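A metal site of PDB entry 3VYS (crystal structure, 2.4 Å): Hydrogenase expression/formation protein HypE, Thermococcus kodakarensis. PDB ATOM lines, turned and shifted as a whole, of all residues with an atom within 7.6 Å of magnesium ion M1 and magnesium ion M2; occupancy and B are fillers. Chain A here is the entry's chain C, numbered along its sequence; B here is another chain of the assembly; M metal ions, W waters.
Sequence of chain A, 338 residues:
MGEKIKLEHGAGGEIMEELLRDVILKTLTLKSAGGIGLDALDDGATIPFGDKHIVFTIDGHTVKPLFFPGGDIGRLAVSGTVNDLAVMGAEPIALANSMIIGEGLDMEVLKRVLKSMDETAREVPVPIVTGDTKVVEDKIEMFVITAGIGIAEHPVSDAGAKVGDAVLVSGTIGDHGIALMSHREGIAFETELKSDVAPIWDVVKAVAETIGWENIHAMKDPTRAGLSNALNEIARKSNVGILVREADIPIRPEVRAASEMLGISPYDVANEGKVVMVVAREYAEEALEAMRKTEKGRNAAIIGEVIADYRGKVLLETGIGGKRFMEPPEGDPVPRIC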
ATOM      1  N   LEU A  41      12.652   7.565  22.389  1.00  0.00           N
ATOM      2  CA  LEU A  41      13.572   6.499  21.999  1.00  0.00           C
ATOM      3  C   LEU A  41      14.035   6.690  20.570  1.00  0.00           C
ATOM      4  O   LEU A  41      14.233   5.722  19.844  1.00  0.00           O
ATOM      5  CB  LEU A  41      12.917   5.124  22.131  1.00  0.00           C
ATOM      6  CG  LEU A  41      12.686   4.615  23.561  1.00  0.00           C
ATOM      7  CD1 LEU A  41      11.949   3.296  23.503  1.00  0.00           C
ATOM      8  CD2 LEU A  41      14.037   4.477  24.275  1.00  0.00           C
ATOM      9  N   ASP A  42      14.184   7.949  20.167  1.00  0.00           N
ATOM     10  CA  ASP A  42      14.625   8.258  18.821  1.00  0.00           C
ATOM     11  C   ASP A  42      16.143   8.093  18.749  1.00  0.00           C
ATOM     12  O   ASP A  42      16.810   7.883  19.766  1.00  0.00           O
ATOM     13  CB  ASP A  42      14.249   9.690  18.453  1.00  0.00           C
ATOM     14  CG  ASP A  42      13.848   9.829  16.993  1.00  0.00           C
ATOM     15  OD1 ASP A  42      12.623   9.848  16.707  1.00  0.00           O
ATOM     16  OD2 ASP A  42      14.746   9.909  16.134  1.00  0.00           O
ATOM     17  N   ASP A  43      16.675   8.209  17.528  1.00  0.00           N
ATOM     18  CA  ASP A  43      18.107   8.082  17.288  1.00  0.00           C
ATOM     19  C   ASP A  43      18.886   9.102  18.096  1.00  0.00           C
ATOM     20  O   ASP A  43      20.103   8.971  18.280  1.00  0.00           O
ATOM     21  CB  ASP A  43      18.376   8.253  15.795  1.00  0.00           C
ATOM     22  CG  ASP A  43      17.743   7.163  14.957  1.00  0.00           C
ATOM     23  OD1 ASP A  43      18.296   6.053  14.895  1.00  0.00           O
ATOM     24  OD2 ASP A  43      16.664   7.414  14.373  1.00  0.00           O
ATOM     25  N   GLY A  44      18.182  10.109  18.585  1.00  0.00           N
ATOM     26  CA  GLY A  44      18.810  11.138  19.378  1.00  0.00           C
ATOM     27  C   GLY A  44      17.742  12.050  19.961  1.00  0.00           C
ATOM     28  O   GLY A  44      16.559  11.873  19.673  1.00  0.00           O
ATOM     29  N   THR A  57      23.161  12.912  21.069  1.00  0.00           N
ATOM     30  CA  THR A  57      23.077  11.483  21.004  1.00  0.00           C
ATOM     31  C   THR A  57      24.331  10.842  21.558  1.00  0.00           C
ATOM     32  O   THR A  57      25.403  11.458  21.577  1.00  0.00           O
ATOM     33  CB  THR A  57      22.883  11.016  19.567  1.00  0.00           C
ATOM     34  OG1 THR A  57      22.615   9.616  19.547  1.00  0.00           O
ATOM     35  CG2 THR A  57      24.132  11.307  18.750  1.00  0.00           C
ATOM     36  N   ILE A  58      24.202   9.598  22.022  1.00  0.00           N
ATOM     37  CA  ILE A  58      25.327   8.853  22.562  1.00  0.00           C
ATOM     38  C   ILE A  58      25.154   7.388  22.166  1.00  0.00           C
ATOM     39  O   ILE A  58      24.031   6.904  22.030  1.00  0.00           O
ATOM     40  CB  ILE A  58      25.401   8.992  24.106  1.00  0.00           C
ATOM     41  CG1 ILE A  58      26.742   8.472  24.599  1.00  0.00           C
ATOM     42  CG2 ILE A  58      24.248   8.243  24.765  1.00  0.00           C
ATOM     43  CD1 ILE A  58      27.036   8.766  26.045  1.00  0.00           C
ATOM     44  N   ASP A  59      26.273   6.693  21.968  1.00  0.00           N
ATOM     45  CA  ASP A  59      26.214   5.292  21.581  1.00  0.00           C
ATOM     46  C   ASP A  59      27.387   4.457  22.101  1.00  0.00           C
ATOM     47  O   ASP A  59      28.553   4.865  22.021  1.00  0.00           O
ATOM     48  CB  ASP A  59      26.164   5.165  20.051  1.00  0.00           C
ATOM     49  CG  ASP A  59      25.125   4.175  19.585  1.00  0.00           C
ATOM     50  OD1 ASP A  59      24.998   3.091  20.202  1.00  0.00           O
ATOM     51  OD2 ASP A  59      24.435   4.459  18.582  1.00  0.00           O
ATOM     52  N   GLY A  60      27.071   3.298  22.650  1.00  0.00           N
ATOM     53  CA  GLY A  60      28.099   2.419  23.151  1.00  0.00           C
ATOM     54  C   GLY A  60      28.459   1.401  22.092  1.00  0.00           C
ATOM     55  O   GLY A  60      27.590   0.899  21.380  1.00  0.00           O
ATOM     56  N   HIS A  61      29.738   1.102  21.960  1.00  0.00           N
ATOM     57  CA  HIS A  61      30.208   0.125  20.981  1.00  0.00           C
ATOM     58  C   HIS A  61      31.018  -0.932  21.680  1.00  0.00           C
ATOM     59  O   HIS A  61      31.951  -0.626  22.439  1.00  0.00           O
ATOM     60  CB  HIS A  61      31.007   0.830  19.903  1.00  0.00           C
ATOM     61  CG  HIS A  61      30.195   1.820  19.137  1.00  0.00           C
ATOM     62  ND1 HIS A  61      29.235   1.455  18.221  1.00  0.00           N
ATOM     63  CD2 HIS A  61      30.119   3.172  19.237  1.00  0.00           C
ATOM     64  CE1 HIS A  61      28.601   2.525  17.792  1.00  0.00           C
ATOM     65  NE2 HIS A  61      29.109   3.586  18.395  1.00  0.00           N
ATOM     66  N   GLY A  80      28.662   5.475  13.735  1.00  0.00           N
ATOM     67  CA  GLY A  80      27.408   5.360  14.449  1.00  0.00           C
ATOM     68  C   GLY A  80      26.855   6.668  14.996  1.00  0.00           C
ATOM     69  O   GLY A  80      25.685   6.971  14.815  1.00  0.00           O
ATOM     70  N   THR A  81      27.700   7.443  15.655  1.00  0.00           N
ATOM     71  CA  THR A  81      27.237   8.709  16.216  1.00  0.00           C
ATOM     72  C   THR A  81      26.876   9.721  15.132  1.00  0.00           C
ATOM     73  O   THR A  81      25.862  10.399  15.233  1.00  0.00           O
ATOM     74  CB  THR A  81      28.291   9.303  17.160  1.00  0.00           C
ATOM     75  OG1 THR A  81      28.612   8.346  18.177  1.00  0.00           O
ATOM     76  CG2 THR A  81      27.741  10.572  17.821  1.00  0.00           C
ATOM     77  N   ASN A  83      25.893   9.029  12.135  1.00  0.00           N
ATOM     78  CA  ASN A  83      24.669   8.591  11.486  1.00  0.00           C
ATOM     79  C   ASN A  83      23.444   8.893  12.335  1.00  0.00           C
ATOM     80  O   ASN A  83      22.426   9.313  11.799  1.00  0.00           O
ATOM     81  CB  ASN A  83      24.742   7.110  11.121  1.00  0.00           C
ATOM     82  CG  ASN A  83      25.721   6.844   9.988  1.00  0.00           C
ATOM     83  OD1 ASN A  83      26.238   7.783   9.363  1.00  0.00           O
ATOM     84  ND2 ASN A  83      25.969   5.570   9.706  1.00  0.00           N
ATOM     85  N   ASP A  84      23.539   8.688  13.638  1.00  0.00           N
ATOM     86  CA  ASP A  84      22.398   8.980  14.506  1.00  0.00           C
ATOM     87  C   ASP A  84      22.051  10.467  14.489  1.00  0.00           C
ATOM     88  O   ASP A  84      20.884  10.825  14.616  1.00  0.00           O
ATOM     89  CB  ASP A  84      22.678   8.517  15.943  1.00  0.00           C
ATOM     90  CG  ASP A  84      22.215   7.094  16.204  1.00  0.00           C
ATOM     91  OD1 ASP A  84      21.140   6.711  15.706  1.00  0.00           O
ATOM     92  OD2 ASP A  84      22.926   6.350  16.918  1.00  0.00           O
ATOM     93  N   LEU A  85      23.047  11.328  14.352  1.00  0.00           N
ATOM     94  CA  LEU A  85      22.771  12.759  14.289  1.00  0.00           C
ATOM     95  C   LEU A  85      22.100  13.039  12.939  1.00  0.00           C
ATOM     96  O   LEU A  85      21.096  13.752  12.864  1.00  0.00           O
ATOM     97  CB  LEU A  85      24.065  13.565  14.388  1.00  0.00           C
ATOM     98  CG  LEU A  85      24.765  13.665  15.757  1.00  0.00           C
ATOM     99  CD1 LEU A  85      26.184  14.166  15.559  1.00  0.00           C
ATOM    100  CD2 LEU A  85      23.979  14.604  16.678  1.00  0.00           C
ATOM    101  N   VAL A  87      20.244  11.084  10.869  1.00  0.00           N
ATOM    102  CA  VAL A  87      18.867  10.652  10.682  1.00  0.00           C
ATOM    103  C   VAL A  87      17.897  11.538  11.463  1.00  0.00           C
ATOM    104  O   VAL A  87      16.677  11.404  11.350  1.00  0.00           O
ATOM    105  CB  VAL A  87      18.653   9.151  11.089  1.00  0.00           C
ATOM    106  CG1 VAL A  87      19.426   8.252  10.133  1.00  0.00           C
ATOM    107  CG2 VAL A  87      19.115   8.912  12.515  1.00  0.00           C
ATOM    108  N   MET A  88      18.449  12.452  12.252  1.00  0.00           N
ATOM    109  CA  MET A  88      17.629  13.386  13.020  1.00  0.00           C
ATOM    110  C   MET A  88      17.487  14.640  12.187  1.00  0.00           C
ATOM    111  O   MET A  88      16.638  15.485  12.464  1.00  0.00           O
ATOM    112  CB  MET A  88      18.296  13.729  14.357  1.00  0.00           C
ATOM    113  CG  MET A  88      18.315  12.605  15.385  1.00  0.00           C
ATOM    114  SD  MET A  88      16.696  11.874  15.630  1.00  0.00           S
ATOM    115  CE  MET A  88      16.020  12.974  16.907  1.00  0.00           C
ATOM    116  N   ASP A 158      10.938   9.739  14.253  1.00  0.00           N
ATOM    117  CA  ASP A 158      10.405   8.463  13.797  1.00  0.00           C
ATOM    118  C   ASP A 158       8.888   8.476  13.704  1.00  0.00           C
ATOM    119  O   ASP A 158       8.286   7.493  13.272  1.00  0.00           O
ATOM    120  CB  ASP A 158      10.815   7.344  14.768  1.00  0.00           C
ATOM    121  CG  ASP A 158      12.302   7.324  15.045  1.00  0.00           C
ATOM    122  OD1 ASP A 158      13.074   7.942  14.281  1.00  0.00           O
ATOM    123  OD2 ASP A 158      12.694   6.678  16.032  1.00  0.00           O
ATOM    124  N   MET A 219      13.334   9.208   9.362  1.00  0.00           N
ATOM    125  CA  MET A 219      14.597   8.532   9.100  1.00  0.00           C
ATOM    126  C   MET A 219      15.033   7.686  10.277  1.00  0.00           C
ATOM    127  O   MET A 219      14.546   7.841  11.395  1.00  0.00           O
ATOM    128  CB  MET A 219      15.701   9.530   8.792  1.00  0.00           C
ATOM    129  CG  MET A 219      15.618  10.199   7.442  1.00  0.00           C
ATOM    130  SD  MET A 219      17.047  11.248   7.187  1.00  0.00           S
ATOM    131  CE  MET A 219      16.680  12.567   8.333  1.00  0.00           C
ATOM    132  N   LYS A 220      15.981   6.789  10.010  1.00  0.00           N
ATOM    133  CA  LYS A 220      16.526   5.911  11.034  1.00  0.00           C
ATOM    134  C   LYS A 220      17.602   5.007  10.432  1.00  0.00           C
ATOM    135  O   LYS A 220      17.423   4.408   9.364  1.00  0.00           O
ATOM    136  CB  LYS A 220      15.429   5.062  11.667  1.00  0.00           C
ATOM    137  CG  LYS A 220      15.943   4.059  12.683  1.00  0.00           C
ATOM    138  CD  LYS A 220      14.831   3.635  13.626  1.00  0.00           C
ATOM    139  CE  LYS A 220      14.417   4.781  14.555  1.00  0.00           C
ATOM    140  NZ  LYS A 220      15.452   5.137  15.568  1.00  0.00           N
ATOM    141  N   ASP A 221      18.742   4.918  11.112  1.00  0.00           N
ATOM    142  CA  ASP A 221      19.815   4.071  10.657  1.00  0.00           C
ATOM    143  C   ASP A 221      19.483   2.703  11.227  1.00  0.00           C
ATOM    144  O   ASP A 221      19.411   2.523  12.443  1.00  0.00           O
ATOM    145  CB  ASP A 221      21.177   4.595  11.150  1.00  0.00           C
ATOM    146  CG  ASP A 221      21.221   4.797  12.645  1.00  0.00           C
ATOM    147  OD1 ASP A 221      20.165   5.128  13.230  1.00  0.00           O
ATOM    148  OD2 ASP A 221      22.308   4.640  13.237  1.00  0.00           O
ATOM    149  N   PRO A 222      19.297   1.724  10.359  1.00  0.00           N
ATOM    150  CA  PRO A 222      18.874   0.411  10.817  1.00  0.00           C
ATOM    151  C   PRO A 222      20.066  -0.382  11.309  1.00  0.00           C
ATOM    152  O   PRO A 222      20.620  -1.191  10.596  1.00  0.00           O
ATOM    153  CB  PRO A 222      18.304  -0.228   9.558  1.00  0.00           C
ATOM    154  CG  PRO A 222      19.002   0.434   8.454  1.00  0.00           C
ATOM    155  CD  PRO A 222      19.234   1.834   8.894  1.00  0.00           C
ATOM    156  N   THR A 223      20.415  -0.150  12.569  1.00  0.00           N
ATOM    157  CA  THR A 223      21.544  -0.807  13.175  1.00  0.00           C
ATOM    158  C   THR A 223      21.098  -2.065  13.900  1.00  0.00           C
ATOM    159  O   THR A 223      20.684  -3.012  13.275  1.00  0.00           O
ATOM    160  CB  THR A 223      22.269   0.126  14.148  1.00  0.00           C
ATOM    161  OG1 THR A 223      21.310   0.733  15.011  1.00  0.00           O
ATOM    162  CG2 THR A 223      22.973   1.216  13.379  1.00  0.00           C
ATOM    163  N   ARG A 224      21.157  -2.078  15.221  1.00  0.00           N
ATOM    164  CA  ARG A 224      20.817  -3.310  15.917  1.00  0.00           C
ATOM    165  C   ARG A 224      19.404  -3.755  15.588  1.00  0.00           C
ATOM    166  O   ARG A 224      18.464  -2.982  15.633  1.00  0.00           O
ATOM    167  CB  ARG A 224      20.953  -3.127  17.426  1.00  0.00           C
ATOM    168  CG  ARG A 224      22.313  -3.497  17.989  1.00  0.00           C
ATOM    169  CD  ARG A 224      22.286  -3.469  19.501  1.00  0.00           C
ATOM    170  NE  ARG A 224      21.999  -2.128  20.003  1.00  0.00           N
ATOM    171  CZ  ARG A 224      21.834  -1.845  21.282  1.00  0.00           C
ATOM    172  NH1 ARG A 224      21.921  -2.795  22.194  1.00  0.00           N
ATOM    173  NH2 ARG A 224      21.569  -0.600  21.664  1.00  0.00           N
ATOM    174  N   GLU A 233       9.803   0.280  14.120  1.00  0.00           N
ATOM    175  CA  GLU A 233       9.840   1.403  15.046  1.00  0.00           C
ATOM    176  C   GLU A 233       9.126   2.601  14.444  1.00  0.00           C
ATOM    177  O   GLU A 233       8.345   3.254  15.119  1.00  0.00           O
ATOM    178  CB  GLU A 233      11.280   1.766  15.401  1.00  0.00           C
ATOM    179  CG  GLU A 233      11.582   1.568  16.886  1.00  0.00           C
ATOM    180  CD  GLU A 233      13.008   1.957  17.265  1.00  0.00           C
ATOM    181  OE1 GLU A 233      13.962   1.297  16.799  1.00  0.00           O
ATOM    182  OE2 GLU A 233      13.163   2.929  18.042  1.00  0.00           O
ATOM    183  N   GLU A 272      25.608  -0.844   9.255  1.00  0.00           N
ATOM    184  CA  GLU A 272      26.349   0.257   9.839  1.00  0.00           C
ATOM    185  C   GLU A 272      26.645   1.384   8.861  1.00  0.00           C
ATOM    186  O   GLU A 272      27.293   2.355   9.205  1.00  0.00           O
ATOM    187  CB  GLU A 272      27.625  -0.250  10.515  1.00  0.00           C
ATOM    188  CG  GLU A 272      27.349  -1.167  11.679  1.00  0.00           C
ATOM    189  CD  GLU A 272      26.553  -0.476  12.771  1.00  0.00           C
ATOM    190  OE1 GLU A 272      26.537   0.757  12.813  1.00  0.00           O
ATOM    191  OE2 GLU A 272      25.956  -1.180  13.598  1.00  0.00           O
ATOM    192  N   GLY B 131      19.912   8.056  25.523  1.00  0.00           N
ATOM    193  CA  GLY B 131      20.738   7.025  26.110  1.00  0.00           C
ATOM    194  C   GLY B 131      21.053   5.859  25.191  1.00  0.00           C
ATOM    195  O   GLY B 131      20.775   5.912  23.987  1.00  0.00           O
ATOM    196  N   ASP B 132      21.657   4.825  25.766  1.00  0.00           N
ATOM    197  CA  ASP B 132      22.016   3.620  25.023  1.00  0.00           C
ATOM    198  C   ASP B 132      22.269   2.500  26.022  1.00  0.00           C
ATOM    199  O   ASP B 132      22.733   2.749  27.141  1.00  0.00           O
ATOM    200  CB  ASP B 132      23.276   3.855  24.194  1.00  0.00           C
ATOM    201  CG  ASP B 132      23.609   2.663  23.313  1.00  0.00           C
ATOM    202  OD1 ASP B 132      22.726   2.236  22.537  1.00  0.00           O
ATOM    203  OD2 ASP B 132      24.752   2.159  23.375  1.00  0.00           O
ATOM    204  N   LYS B 134      23.910  -1.494  26.305  1.00  0.00           N
ATOM    205  CA  LYS B 134      24.610  -2.642  25.755  1.00  0.00           C
ATOM    206  C   LYS B 134      24.728  -3.703  26.841  1.00  0.00           C
ATOM    207  O   LYS B 134      24.762  -3.380  28.031  1.00  0.00           O
ATOM    208  CB  LYS B 134      26.001  -2.238  25.283  1.00  0.00           C
ATOM    209  CG  LYS B 134      26.012  -1.415  24.004  1.00  0.00           C
ATOM    210  CD  LYS B 134      25.490  -2.224  22.817  1.00  0.00           C
ATOM    211  CE  LYS B 134      25.646  -1.471  21.507  1.00  0.00           C
ATOM    212  NZ  LYS B 134      24.871  -0.193  21.469  1.00  0.00           N
HETATM  213 MG    MG M   1      19.905   5.082  15.556  1.00  0.00          MG
HETATM  214 MG    MG M   2      22.694   3.954  17.062  1.00  0.00          MG
HETATM  215 MG    MG M   3      14.831   9.249  13.509  1.00  0.00          MG
HETATM  216  O   HOH W   1      21.940   3.712  20.210  1.00  0.00           O
HETATM  217  O   HOH W   2      22.459   1.248  18.144  1.00  0.00           O
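Magnesium ion M2 is bound by the side-chain carboxylate of Asp 59 (2.4 Å) and the side-chain carboxylate of Asp 84 (2.4 Å).
Of the 28 residues printed, 3 come within 4 Å of magnesium ion M1.
Water W1 bridges OD1 of Asp 132 of chain B (2.9 Å) and OD1 of Asp 59 (3.1 Å).
Three residues have an atom within 4 Å of magnesium ion M2: Asp 59, Asp 84 and Asp 221.
The nearest printed residue that does not touch magnesium ion M2 is Thr 223 (4.1 Å).
Magnesium ion M1 is bound by OD1 of Asp 43 (2.0 Å), OD1 of Asp 84 (2.0 Å) and OD1 of Asp 221 (2.3 Å).
Magnesium ion M1 has three donor atoms within binding distance.
NZ of Lys 220 lies within salt-bridge range of OD2 of Asp 43, 2.8 Å away.
The backbone carbonyl oxygen (O) of Asp 43 sits at hydrogen-bond distance from the side-chain hydroxyl (OG1) of Thr 57 (2.9 Å).
The side-chain carboxylate of Asp 59 lies within salt-bridge range of the side-chain amino group of Lys 134 of chain B, at 3.5 Å.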
